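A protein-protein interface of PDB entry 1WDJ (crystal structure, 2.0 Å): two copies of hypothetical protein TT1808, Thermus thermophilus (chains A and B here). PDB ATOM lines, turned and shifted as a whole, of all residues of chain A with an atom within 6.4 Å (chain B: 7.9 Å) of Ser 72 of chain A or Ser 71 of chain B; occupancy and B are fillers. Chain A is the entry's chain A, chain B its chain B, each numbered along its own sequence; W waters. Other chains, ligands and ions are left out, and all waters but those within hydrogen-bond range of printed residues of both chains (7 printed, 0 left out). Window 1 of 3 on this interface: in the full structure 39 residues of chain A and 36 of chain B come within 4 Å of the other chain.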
ATOM      1  N   SER A  20     -23.520  25.721  18.172  1.00  0.00           N
ATOM      2  CA  SER A  20     -24.407  26.004  19.304  1.00  0.00           C
ATOM      3  C   SER A  20     -24.675  27.490  19.320  1.00  0.00           C
ATOM      4  O   SER A  20     -25.814  27.933  19.506  1.00  0.00           O
ATOM      5  CB  SER A  20     -23.766  25.600  20.632  1.00  0.00           C
ATOM      6  OG  SER A  20     -23.657  24.190  20.731  1.00  0.00           O
ATOM      7  N   GLY A  25     -31.293  27.202  20.952  1.00  0.00           N
ATOM      8  CA  GLY A  25     -32.417  26.272  20.988  1.00  0.00           C
ATOM      9  C   GLY A  25     -32.106  24.894  20.413  1.00  0.00           C
ATOM     10  O   GLY A  25     -32.940  23.989  20.440  1.00  0.00           O
ATOM     11  N   GLN A  27     -29.462  21.504  20.258  1.00  0.00           N
ATOM     12  CA  GLN A  27     -28.424  20.753  20.922  1.00  0.00           C
ATOM     13  C   GLN A  27     -27.585  20.048  19.857  1.00  0.00           C
ATOM     14  O   GLN A  27     -28.110  19.294  19.021  1.00  0.00           O
ATOM     15  CB  GLN A  27     -29.059  19.726  21.835  1.00  0.00           C
ATOM     16  CG  GLN A  27     -28.062  18.802  22.453  1.00  0.00           C
ATOM     17  CD  GLN A  27     -28.716  17.858  23.399  1.00  0.00           C
ATOM     18  OE1 GLN A  27     -28.849  16.667  23.118  1.00  0.00           O
ATOM     19  NE2 GLN A  27     -29.155  18.385  24.535  1.00  0.00           N
ATOM     20  N   LEU A  50     -35.500  20.855  33.112  1.00  0.00           N
ATOM     21  CA  LEU A  50     -35.257  21.786  34.216  1.00  0.00           C
ATOM     22  C   LEU A  50     -35.735  21.124  35.511  1.00  0.00           C
ATOM     23  O   LEU A  50     -34.991  21.040  36.501  1.00  0.00           O
ATOM     24  CB  LEU A  50     -36.014  23.101  33.983  1.00  0.00           C
ATOM     25  CG  LEU A  50     -36.060  24.202  35.067  1.00  0.00           C
ATOM     26  CD1 LEU A  50     -37.020  23.812  36.205  1.00  0.00           C
ATOM     27  CD2 LEU A  50     -34.646  24.464  35.602  1.00  0.00           C
ATOM     28  N   PHE A  69     -24.941  19.277  36.350  1.00  0.00           N
ATOM     29  CA  PHE A  69     -24.912  20.125  35.159  1.00  0.00           C
ATOM     30  C   PHE A  69     -26.268  20.118  34.486  1.00  0.00           C
ATOM     31  O   PHE A  69     -26.975  19.111  34.545  1.00  0.00           O
ATOM     32  CB  PHE A  69     -23.856  19.601  34.168  1.00  0.00           C
ATOM     33  CG  PHE A  69     -22.479  19.478  34.769  1.00  0.00           C
ATOM     34  CD1 PHE A  69     -22.148  18.392  35.558  1.00  0.00           C
ATOM     35  CD2 PHE A  69     -21.528  20.469  34.569  1.00  0.00           C
ATOM     36  CE1 PHE A  69     -20.884  18.296  36.145  1.00  0.00           C
ATOM     37  CE2 PHE A  69     -20.274  20.383  35.148  1.00  0.00           C
ATOM     38  CZ  PHE A  69     -19.952  19.292  35.940  1.00  0.00           C
ATOM     39  N   ASP A  70     -26.652  21.231  33.866  1.00  0.00           N
ATOM     40  CA  ASP A  70     -27.941  21.241  33.187  1.00  0.00           C
ATOM     41  C   ASP A  70     -27.818  20.678  31.772  1.00  0.00           C
ATOM     42  O   ASP A  70     -26.728  20.301  31.333  1.00  0.00           O
ATOM     43  CB  ASP A  70     -28.579  22.637  33.173  1.00  0.00           C
ATOM     44  CG  ASP A  70     -27.754  23.672  32.439  1.00  0.00           C
ATOM     45  OD1 ASP A  70     -26.831  23.319  31.676  1.00  0.00           O
ATOM     46  OD2 ASP A  70     -28.060  24.865  32.630  1.00  0.00           O
ATOM     47  N   SER A  71     -28.938  20.639  31.068  1.00  0.00           N
ATOM     48  CA  SER A  71     -29.009  20.054  29.741  1.00  0.00           C
ATOM     49  C   SER A  71     -28.210  20.663  28.597  1.00  0.00           C
ATOM     50  O   SER A  71     -28.156  20.085  27.516  1.00  0.00           O
ATOM     51  CB  SER A  71     -30.472  19.965  29.315  1.00  0.00           C
ATOM     52  OG  SER A  71     -31.032  21.263  29.209  1.00  0.00           O
ATOM     53  N   SER A  72     -27.585  21.811  28.795  1.00  0.00           N
ATOM     54  CA  SER A  72     -26.850  22.415  27.678  1.00  0.00           C
ATOM     55  C   SER A  72     -25.407  21.950  27.646  1.00  0.00           C
ATOM     56  O   SER A  72     -24.654  22.256  26.708  1.00  0.00           O
ATOM     57  CB  SER A  72     -26.900  23.949  27.776  1.00  0.00           C
ATOM     58  OG  SER A  72     -26.248  24.418  28.960  1.00  0.00           O
ATOM     59  N   THR A  73     -25.031  21.187  28.670  1.00  0.00           N
ATOM     60  CA  THR A  73     -23.661  20.704  28.798  1.00  0.00           C
ATOM     61  C   THR A  73     -23.350  19.451  27.980  1.00  0.00           C
ATOM     62  O   THR A  73     -24.118  18.485  27.974  1.00  0.00           O
ATOM     63  CB  THR A  73     -23.334  20.425  30.279  1.00  0.00           C
ATOM     64  OG1 THR A  73     -23.763  21.536  31.074  1.00  0.00           O
ATOM     65  CG2 THR A  73     -21.846  20.201  30.490  1.00  0.00           C
ATOM     66  N   GLY A  74     -22.223  19.487  27.275  1.00  0.00           N
ATOM     67  CA  GLY A  74     -21.789  18.341  26.488  1.00  0.00           C
ATOM     68  C   GLY A  74     -20.558  17.717  27.141  1.00  0.00           C
ATOM     69  O   GLY A  74     -19.687  18.425  27.612  1.00  0.00           O
ATOM     70  N   SER A  84     -24.722  15.227  25.116  1.00  0.00           N
ATOM     71  CA  SER A  84     -25.330  16.169  26.052  1.00  0.00           C
ATOM     72  C   SER A  84     -26.650  15.662  26.658  1.00  0.00           C
ATOM     73  O   SER A  84     -27.717  15.829  26.072  1.00  0.00           O
ATOM     74  CB  SER A  84     -25.555  17.507  25.329  1.00  0.00           C
ATOM     75  OG  SER A  84     -26.278  18.429  26.129  1.00  0.00           O
ATOM     76  N   PRO A  85     -26.591  15.035  27.843  1.00  0.00           N
ATOM     77  CA  PRO A  85     -27.843  14.551  28.438  1.00  0.00           C
ATOM     78  C   PRO A  85     -28.677  15.717  28.970  1.00  0.00           C
ATOM     79  O   PRO A  85     -28.254  16.866  28.898  1.00  0.00           O
ATOM     80  CB  PRO A  85     -27.352  13.626  29.564  1.00  0.00           C
ATOM     81  CG  PRO A  85     -26.052  14.270  29.997  1.00  0.00           C
ATOM     82  CD  PRO A  85     -25.420  14.707  28.686  1.00  0.00           C
ATOM     83  N   ASP A  86     -29.869  15.426  29.496  1.00  0.00           N
ATOM     84  CA  ASP A  86     -30.705  16.470  30.073  1.00  0.00           C
ATOM     85  C   ASP A  86     -30.194  16.822  31.481  1.00  0.00           C
ATOM     86  O   ASP A  86     -30.456  17.901  31.997  1.00  0.00           O
ATOM     87  CB  ASP A  86     -32.171  16.019  30.112  1.00  0.00           C
ATOM     88  CG  ASP A  86     -32.795  15.989  28.718  1.00  0.00           C
ATOM     89  OD1 ASP A  86     -32.697  17.014  28.018  1.00  0.00           O
ATOM     90  OD2 ASP A  86     -33.372  14.962  28.318  1.00  0.00           O
ATOM     91  N   PHE A 106     -15.728  20.908  26.903  1.00  0.00           N
ATOM     92  CA  PHE A 106     -16.559  19.724  27.124  1.00  0.00           C
ATOM     93  C   PHE A 106     -15.754  18.791  28.009  1.00  0.00           C
ATOM     94  O   PHE A 106     -14.790  18.173  27.555  1.00  0.00           O
ATOM     95  CB  PHE A 106     -16.873  19.028  25.807  1.00  0.00           C
ATOM     96  CG  PHE A 106     -17.510  19.919  24.795  1.00  0.00           C
ATOM     97  CD1 PHE A 106     -16.846  20.247  23.622  1.00  0.00           C
ATOM     98  CD2 PHE A 106     -18.794  20.414  24.998  1.00  0.00           C
ATOM     99  CE1 PHE A 106     -17.453  21.053  22.662  1.00  0.00           C
ATOM    100  CE2 PHE A 106     -19.413  21.217  24.050  1.00  0.00           C
ATOM    101  CZ  PHE A 106     -18.743  21.538  22.876  1.00  0.00           C
ATOM    102  N   SER B  39     -16.444  27.235  26.229  1.00  0.00           N
ATOM    103  CA  SER B  39     -17.681  26.970  25.512  1.00  0.00           C
ATOM    104  C   SER B  39     -18.907  27.253  26.377  1.00  0.00           C
ATOM    105  O   SER B  39     -18.929  26.931  27.564  1.00  0.00           O
ATOM    106  CB  SER B  39     -17.735  25.517  25.033  1.00  0.00           C
ATOM    107  OG  SER B  39     -18.893  25.289  24.236  1.00  0.00           O
ATOM    108  N   PRO B  40     -19.929  27.900  25.792  1.00  0.00           N
ATOM    109  CA  PRO B  40     -21.175  28.222  26.501  1.00  0.00           C
ATOM    110  C   PRO B  40     -21.876  26.904  26.852  1.00  0.00           C
ATOM    111  O   PRO B  40     -22.701  26.841  27.766  1.00  0.00           O
ATOM    112  CB  PRO B  40     -21.959  29.034  25.474  1.00  0.00           C
ATOM    113  CG  PRO B  40     -20.868  29.724  24.709  1.00  0.00           C
ATOM    114  CD  PRO B  40     -19.854  28.623  24.510  1.00  0.00           C
ATOM    115  N   THR B  41     -21.518  25.857  26.112  1.00  0.00           N
ATOM    116  CA  THR B  41     -22.067  24.513  26.307  1.00  0.00           C
ATOM    117  C   THR B  41     -21.049  23.597  27.000  1.00  0.00           C
ATOM    118  O   THR B  41     -21.158  22.375  26.915  1.00  0.00           O
ATOM    119  CB  THR B  41     -22.472  23.870  24.941  1.00  0.00           C
ATOM    120  OG1 THR B  41     -21.375  23.976  24.020  1.00  0.00           O
ATOM    121  CG2 THR B  41     -23.681  24.585  24.340  1.00  0.00           C
ATOM    122  N   GLY B  42     -20.068  24.201  27.680  1.00  0.00           N
ATOM    123  CA  GLY B  42     -19.034  23.452  28.397  1.00  0.00           C
ATOM    124  C   GLY B  42     -19.396  23.216  29.868  1.00  0.00           C
ATOM    125  O   GLY B  42     -20.459  23.638  30.329  1.00  0.00           O
ATOM    126  N   GLY B  43     -18.506  22.561  30.612  1.00  0.00           N
ATOM    127  CA  GLY B  43     -18.771  22.254  32.007  1.00  0.00           C
ATOM    128  C   GLY B  43     -19.043  23.413  32.959  1.00  0.00           C
ATOM    129  O   GLY B  43     -20.096  23.465  33.602  1.00  0.00           O
ATOM    130  N   SER B  45     -19.838  26.571  32.470  1.00  0.00           N
ATOM    131  CA  SER B  45     -21.058  27.312  32.147  1.00  0.00           C
ATOM    132  C   SER B  45     -22.275  26.490  32.582  1.00  0.00           C
ATOM    133  O   SER B  45     -23.223  27.033  33.162  1.00  0.00           O
ATOM    134  CB  SER B  45     -21.155  27.608  30.638  1.00  0.00           C
ATOM    135  OG  SER B  45     -20.122  28.472  30.193  1.00  0.00           O
ATOM    136  N   GLY B  46     -22.220  25.182  32.307  1.00  0.00           N
ATOM    137  CA  GLY B  46     -23.304  24.272  32.649  1.00  0.00           C
ATOM    138  C   GLY B  46     -23.521  24.177  34.143  1.00  0.00           C
ATOM    139  O   GLY B  46     -24.665  24.129  34.617  1.00  0.00           O
ATOM    140  N   ARG B  47     -22.418  24.139  34.886  1.00  0.00           N
ATOM    141  CA  ARG B  47     -22.472  24.074  36.344  1.00  0.00           C
ATOM    142  C   ARG B  47     -23.104  25.359  36.907  1.00  0.00           C
ATOM    143  O   ARG B  47     -23.917  25.316  37.832  1.00  0.00           O
ATOM    144  CB  ARG B  47     -21.059  23.915  36.906  1.00  0.00           C
ATOM    145  CG  ARG B  47     -20.984  23.988  38.415  1.00  0.00           C
ATOM    146  CD  ARG B  47     -19.545  23.825  38.896  1.00  0.00           C
ATOM    147  NE  ARG B  47     -18.733  25.013  38.649  1.00  0.00           N
ATOM    148  CZ  ARG B  47     -18.868  26.160  39.309  1.00  0.00           C
ATOM    149  NH1 ARG B  47     -19.789  26.274  40.260  1.00  0.00           N
ATOM    150  NH2 ARG B  47     -18.077  27.187  39.029  1.00  0.00           N
ATOM    151  N   SER B  49     -25.100  27.725  35.205  1.00  0.00           N
ATOM    152  CA  SER B  49     -26.493  27.911  34.833  1.00  0.00           C
ATOM    153  C   SER B  49     -27.393  26.965  35.639  1.00  0.00           C
ATOM    154  O   SER B  49     -28.511  27.343  36.008  1.00  0.00           O
ATOM    155  CB  SER B  49     -26.698  27.718  33.313  1.00  0.00           C
ATOM    156  OG  SER B  49     -26.193  26.469  32.862  1.00  0.00           O
ATOM    157  N   LEU B  50     -26.926  25.749  35.926  1.00  0.00           N
ATOM    158  CA  LEU B  50     -27.760  24.837  36.709  1.00  0.00           C
ATOM    159  C   LEU B  50     -27.977  25.386  38.123  1.00  0.00           C
ATOM    160  O   LEU B  50     -29.075  25.282  38.675  1.00  0.00           O
ATOM    161  CB  LEU B  50     -27.152  23.423  36.800  1.00  0.00           C
ATOM    162  CG  LEU B  50     -28.010  22.499  37.691  1.00  0.00           C
ATOM    163  CD1 LEU B  50     -28.425  21.260  36.928  1.00  0.00           C
ATOM    164  CD2 LEU B  50     -27.234  22.133  38.961  1.00  0.00           C
ATOM    165  N   ALA B  53     -30.547  28.117  37.697  1.00  0.00           N
ATOM    166  CA  ALA B  53     -31.837  27.513  37.386  1.00  0.00           C
ATOM    167  C   ALA B  53     -32.410  26.789  38.600  1.00  0.00           C
ATOM    168  O   ALA B  53     -33.613  26.867  38.875  1.00  0.00           O
ATOM    169  CB  ALA B  53     -31.699  26.547  36.189  1.00  0.00           C
ATOM    170  N   PHE B  69     -37.858  27.194  32.689  1.00  0.00           N
ATOM    171  CA  PHE B  69     -37.183  26.391  31.682  1.00  0.00           C
ATOM    172  C   PHE B  69     -35.687  26.483  31.857  1.00  0.00           C
ATOM    173  O   PHE B  69     -35.194  27.479  32.408  1.00  0.00           O
ATOM    174  CB  PHE B  69     -37.575  26.882  30.281  1.00  0.00           C
ATOM    175  CG  PHE B  69     -39.060  27.030  30.091  1.00  0.00           C
ATOM    176  CD1 PHE B  69     -39.742  28.097  30.673  1.00  0.00           C
ATOM    177  CD2 PHE B  69     -39.780  26.080  29.372  1.00  0.00           C
ATOM    178  CE1 PHE B  69     -41.127  28.217  30.550  1.00  0.00           C
ATOM    179  CE2 PHE B  69     -41.163  26.180  29.238  1.00  0.00           C
ATOM    180  CZ  PHE B  69     -41.844  27.258  29.833  1.00  0.00           C
ATOM    181  N   ASP B  70     -34.970  25.471  31.364  1.00  0.00           N
ATOM    182  CA  ASP B  70     -33.517  25.447  31.476  1.00  0.00           C
ATOM    183  C   ASP B  70     -32.763  26.070  30.301  1.00  0.00           C
ATOM    184  O   ASP B  70     -33.360  26.527  29.320  1.00  0.00           O
ATOM    185  CB  ASP B  70     -33.010  24.019  31.753  1.00  0.00           C
ATOM    186  CG  ASP B  70     -33.114  23.092  30.555  1.00  0.00           C
ATOM    187  OD1 ASP B  70     -32.965  21.869  30.773  1.00  0.00           O
ATOM    188  OD2 ASP B  70     -33.321  23.549  29.410  1.00  0.00           O
ATOM    189  N   SER B  71     -31.442  26.101  30.434  1.00  0.00           N
ATOM    190  CA  SER B  71     -30.545  26.693  29.439  1.00  0.00           C
ATOM    191  C   SER B  71     -30.635  26.166  28.000  1.00  0.00           C
ATOM    192  O   SER B  71     -30.095  26.777  27.083  1.00  0.00           O
ATOM    193  CB  SER B  71     -29.106  26.536  29.927  1.00  0.00           C
ATOM    194  OG  SER B  71     -28.873  25.165  30.232  1.00  0.00           O
ATOM    195  N   SER B  72     -31.306  25.044  27.795  1.00  0.00           N
ATOM    196  CA  SER B  72     -31.415  24.472  26.449  1.00  0.00           C
ATOM    197  C   SER B  72     -32.581  25.028  25.643  1.00  0.00           C
ATOM    198  O   SER B  72     -32.533  25.071  24.405  1.00  0.00           O
ATOM    199  CB  SER B  72     -31.594  22.950  26.536  1.00  0.00           C
ATOM    200  OG  SER B  72     -30.388  22.291  26.879  1.00  0.00           O
ATOM    201  N   THR B  73     -33.624  25.442  26.358  1.00  0.00           N
ATOM    202  CA  THR B  73     -34.845  25.921  25.746  1.00  0.00           C
ATOM    203  C   THR B  73     -34.695  27.077  24.793  1.00  0.00           C
ATOM    204  O   THR B  73     -34.020  28.057  25.088  1.00  0.00           O
ATOM    205  CB  THR B  73     -35.875  26.349  26.810  1.00  0.00           C
ATOM    206  OG1 THR B  73     -35.861  25.421  27.905  1.00  0.00           O
ATOM    207  CG2 THR B  73     -37.273  26.390  26.190  1.00  0.00           C
ATOM    208  N   GLY B  74     -35.364  26.961  23.651  1.00  0.00           N
ATOM    209  CA  GLY B  74     -35.325  28.032  22.680  1.00  0.00           C
ATOM    210  C   GLY B  74     -36.701  28.665  22.695  1.00  0.00           C
ATOM    211  O   GLY B  74     -37.708  27.958  22.800  1.00  0.00           O
ATOM    212  N   PHE B  75     -36.752  29.987  22.616  1.00  0.00           N
ATOM    213  CA  PHE B  75     -38.022  30.700  22.585  1.00  0.00           C
ATOM    214  C   PHE B  75     -38.092  31.490  21.275  1.00  0.00           C
ATOM    215  O   PHE B  75     -37.072  32.000  20.805  1.00  0.00           O
ATOM    216  CB  PHE B  75     -38.132  31.686  23.772  1.00  0.00           C
ATOM    217  CG  PHE B  75     -38.236  31.021  25.124  1.00  0.00           C
ATOM    218  CD1 PHE B  75     -37.090  30.662  25.833  1.00  0.00           C
ATOM    219  CD2 PHE B  75     -39.487  30.731  25.673  1.00  0.00           C
ATOM    220  CE1 PHE B  75     -37.183  30.015  27.078  1.00  0.00           C
ATOM    221  CE2 PHE B  75     -39.596  30.084  26.918  1.00  0.00           C
ATOM    222  CZ  PHE B  75     -38.436  29.727  27.615  1.00  0.00           C
ATOM    223  N   LEU B  83     -34.164  32.684  20.673  1.00  0.00           N
ATOM    224  CA  LEU B  83     -33.131  33.010  21.651  1.00  0.00           C
ATOM    225  C   LEU B  83     -33.228  32.004  22.789  1.00  0.00           C
ATOM    226  O   LEU B  83     -34.313  31.518  23.110  1.00  0.00           O
ATOM    227  CB  LEU B  83     -33.325  34.436  22.174  1.00  0.00           C
ATOM    228  CG  LEU B  83     -33.266  35.526  21.099  1.00  0.00           C
ATOM    229  CD1 LEU B  83     -33.763  36.819  21.704  1.00  0.00           C
ATOM    230  CD2 LEU B  83     -31.850  35.666  20.550  1.00  0.00           C
ATOM    231  N   SER B  84     -32.093  31.704  23.404  1.00  0.00           N
ATOM    232  CA  SER B  84     -32.059  30.723  24.488  1.00  0.00           C
ATOM    233  C   SER B  84     -31.240  31.200  25.687  1.00  0.00           C
ATOM    234  O   SER B  84     -30.016  31.079  25.691  1.00  0.00           O
ATOM    235  CB  SER B  84     -31.460  29.407  23.968  1.00  0.00           C
ATOM    236  OG  SER B  84     -31.368  28.437  25.001  1.00  0.00           O
ATOM    237  N   PRO B  85     -31.899  31.775  26.704  1.00  0.00           N
ATOM    238  CA  PRO B  85     -31.165  32.239  27.893  1.00  0.00           C
ATOM    239  C   PRO B  85     -30.711  31.035  28.746  1.00  0.00           C
ATOM    240  O   PRO B  85     -30.999  29.876  28.388  1.00  0.00           O
ATOM    241  CB  PRO B  85     -32.201  33.094  28.629  1.00  0.00           C
ATOM    242  CG  PRO B  85     -33.483  32.437  28.283  1.00  0.00           C
ATOM    243  CD  PRO B  85     -33.326  32.141  26.792  1.00  0.00           C
ATOM    244  N   ASP B  86     -30.001  31.303  29.852  1.00  0.00           N
ATOM    245  CA  ASP B  86     -29.582  30.224  30.753  1.00  0.00           C
ATOM    246  C   ASP B  86     -30.738  29.709  31.618  1.00  0.00           C
ATOM    247  O   ASP B  86     -30.688  28.592  32.138  1.00  0.00           O
ATOM    248  CB  ASP B  86     -28.416  30.677  31.628  1.00  0.00           C
ATOM    249  CG  ASP B  86     -27.118  30.710  30.853  1.00  0.00           C
ATOM    250  OD1 ASP B  86     -26.846  29.710  30.160  1.00  0.00           O
ATOM    251  OD2 ASP B  86     -26.384  31.716  30.921  1.00  0.00           O
ATOM    252  N   ALA B  87     -31.780  30.533  31.755  1.00  0.00           N
ATOM    253  CA  ALA B  87     -32.979  30.165  32.500  1.00  0.00           C
ATOM    254  C   ALA B  87     -34.083  31.148  32.142  1.00  0.00           C
ATOM    255  O   ALA B  87     -33.816  32.308  31.787  1.00  0.00           O
ATOM    256  CB  ALA B  87     -32.719  30.183  34.009  1.00  0.00           C
ATOM    257  N   ALA B  88     -35.327  30.684  32.220  1.00  0.00           N
ATOM    258  CA  ALA B  88     -36.461  31.537  31.910  1.00  0.00           C
ATOM    259  C   ALA B  88     -37.700  31.184  32.731  1.00  0.00           C
ATOM    260  O   ALA B  88     -37.928  30.028  33.101  1.00  0.00           O
ATOM    261  CB  ALA B  88     -36.788  31.472  30.402  1.00  0.00           C
ATOM    262  N   PHE B 115     -32.614  35.005  32.327  1.00  0.00           N
ATOM    263  CA  PHE B 115     -31.346  35.031  33.033  1.00  0.00           C
ATOM    264  C   PHE B 115     -30.208  34.601  32.095  1.00  0.00           C
ATOM    265  O   PHE B 115     -30.339  33.633  31.334  1.00  0.00           O
ATOM    266  CB  PHE B 115     -31.378  34.071  34.237  1.00  0.00           C
ATOM    267  CG  PHE B 115     -32.398  34.427  35.297  1.00  0.00           C
ATOM    268  CD1 PHE B 115     -33.755  34.155  35.105  1.00  0.00           C
ATOM    269  CD2 PHE B 115     -31.997  35.031  36.494  1.00  0.00           C
ATOM    270  CE1 PHE B 115     -34.704  34.478  36.087  1.00  0.00           C
ATOM    271  CE2 PHE B 115     -32.937  35.359  37.489  1.00  0.00           C
ATOM    272  CZ  PHE B 115     -34.297  35.082  37.280  1.00  0.00           C
ATOM    273  N   GLU B 116     -29.105  35.334  32.157  1.00  0.00           N
ATOM    274  CA  GLU B 116     -27.927  35.023  31.358  1.00  0.00           C
ATOM    275  C   GLU B 116     -26.748  34.996  32.329  1.00  0.00           C
ATOM    276  O   GLU B 116     -26.567  35.926  33.130  1.00  0.00           O
ATOM    277  CB  GLU B 116     -27.701  36.104  30.299  1.00  0.00           C
ATOM    278  CG  GLU B 116     -28.793  36.169  29.237  1.00  0.00           C
ATOM    279  CD  GLU B 116     -28.723  35.019  28.235  1.00  0.00           C
ATOM    280  OE1 GLU B 116     -27.866  34.128  28.406  1.00  0.00           O
ATOM    281  OE2 GLU B 116     -29.532  35.006  27.277  1.00  0.00           O
HETATM  282  O   HOH W   1     -31.211  20.888  32.787  1.00  0.00           O
HETATM  283  O   HOH W   2     -22.941  24.193  29.343  1.00  0.00           O
HETATM  284  O   HOH W   3     -30.505  25.798  33.006  1.00  0.00           O
HETATM  285  O   HOH W   4     -30.265  23.285  22.991  1.00  0.00           O
HETATM  286  O   HOH W   5     -21.691  22.774  21.840  1.00  0.00           O
HETATM  287  O   HOH W   6     -25.814  27.137  27.135  1.00  0.00           O
HETATM  288  O   HOH W   7     -29.219  21.131  24.748  1.00  0.00           O
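OD2 of Asp 70 of chain A is in hydrogen-bond range of OG of Ser 49 of chain B (2.5 Å).
The side-chain carboxylate of Asp 70 of chain A is in hydrogen-bond range of the side-chain hydroxyl of Ser 71 of chain B (2.5 Å).
The side-chain hydroxyl of Ser 71 of chain A is in hydrogen-bond range of the side-chain carboxylate of Asp 70 of chain B (2.6 Å).
The side-chain hydroxyl (OG) of Ser 71 of chain A sits at hydrogen-bond distance from the side-chain hydroxyl (OG) of Ser 72 of chain B.
The side-chain hydroxyl (OG) of Ser 71 of chain B sits at hydrogen-bond distance from the side-chain hydroxyl (OG) of Ser 72 of chain A (3.0 Å).
N of Ser 72 of chain A sits at hydrogen-bond distance from OG of Ser 72 of chain B, 3.4 Å away.
O of Thr 41 of chain B lies within hydrogen-bond range of N of Gly 74 of chain A, 3.1 Å away.
The backbone NH of Ser 71 of chain A sits at hydrogen-bond distance from the backbone carbonyl oxygen of Asp 86 of chain A, at 3.3 Å.
O of Gly 46 of chain B is in hydrogen-bond range of OG of Ser 49 of chain B (3.3 Å).
The backbone NH of Phe 69 of chain B is in hydrogen-bond range of the backbone carbonyl oxygen of Ala 88 of chain B (2.9 Å).
O of Asp 70 of chain B lies within hydrogen-bond range of OG1 of Thr 73 of chain B (3.1 Å).
The backbone NH of Ser 71 of chain B sits at hydrogen-bond distance from the backbone carbonyl oxygen of Asp 86 of chain B, 3.1 Å away.
OG of Ser 84 of chain B is in hydrogen-bond range of O of Thr 73 of chain B, at 2.7 Å.
Ser 20 of chain A touches Thr 41 of chain B.
Ala 53 of chain B touches Leu 50 of chain A (CB to CD2, 3.7 Å).
Asp 70 of chain B touches Leu 50 of chain A.
CE2 of Phe 69 of chain A touches O of Gly 43 of chain B (3.5 Å).
Phe 69 of chain A touches Arg 47 of chain B (CD2 to N, 3.8 Å).
Phe 69 of chain A touches Leu 50 of chain B.
N of Asp 70 of chain A touches CD1 of Leu 50 of chain B, 3.5 Å away.
Ser 72 of chain A touches Thr 41 of chain B (O to CB, 3.2 Å).
CG2 of Thr 73 of chain A touches O of Gly 42 of chain B, at 3.7 Å.
Thr 73 of chain A touches Gly 43 of chain B (CG2 to CA, 3.996 Å).
Printed residues of chain B within 4 Å of Gly 25 of chain A: Ser 72 (3.6 Å), Gly 74 (3.8 Å) and Ser 84 (3.7 Å).
Gln 27 of chain A touches none of the printed residues of chain B.
Of the printed residues of chain B, Phe 69 of chain A touches Gly 43, Arg 47 and Leu 50.
Of chain B, only Thr 41, Ser 71 and Ser 72 come within 4 Å of Ser 72 of chain A.
Of the printed residues of chain B, Gly 74 of chain A touches Thr 41 (3.1 Å).
Of the printed residues of chain A, Ser 39 of chain B touches Phe 106 (3.99 Å).
Ser 71 of chain B touches just these residues of chain A: Asp 70 and Ser 72.
Of the printed residues of chain A, Gly 74 of chain B touches Gly 25 (3.8 Å).
The nearest residue of chain B that does not touch Ser 72 of chain A is Ser 49 of chain B (4.4 Å).
Printed residues of chain B that touch a printed residue of chain A: Ser 39, Thr 41, Gly 42, Gly 43, Gly 46, Arg 47, Ser 49, Leu 50, Ala 53, Phe 69, Asp 70, Ser 71, Ser 72, Gly 74 and Ser 84.
Hydrophobic or aromatic side chains of chain B that line the printed part of chain A: Leu 50 and Ala 53.
Among the printed residues, no Asp or Glu carboxylate lies within 4 Å of a Lys or Arg side-chain nitrogen of the other chain.
Leu 50 of chain A touches Phe 69 of chain B, and with the chains exchanged Phe 69 of chain A touches Leu 50 of chain B.
Asp 70 of chain A touches Ser 71 of chain B, and with the chains exchanged Ser 71 of chain A touches Asp 70 of chain B.
Ser 71 of chain A touches Ser 72 of chain B, and with the chains exchanged Ser 72 of chain A touches Ser 71 of chain B.
Ser 72 of chain B touches its own counterpart, Ser 72 of chain A.
Water W5 bridges OG1 of Thr 41 of chain B and OG of Ser 20 of chain A.
Water W3 lies within hydrogen-bond range of OD2 of Asp 70 of chain A, N of Ser 71 of chain B and O of Asp 86 of chain B.
Water W7 lies within hydrogen-bond range of the side-chain hydroxyl (OG) of Ser 72 of chain B (2.7 Å), the side-chain amide nitrogen (NE2) of Gln 27 of chain A (2.8 Å) and the backbone carbonyl oxygen (O) of Ser 71 of chain A (3.1 Å).
Water W6 lies within hydrogen-bond range of the backbone carbonyl oxygen of Pro 40 of chain B (3.2 Å) and the side-chain hydroxyl of Ser 72 of chain A (3.3 Å).
Water W4 lies within hydrogen-bond range of the backbone carbonyl oxygen (O) of Ser 72 of chain B (3.2 Å) and the backbone NH (N) of Gln 27 of chain A (3.4 Å).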
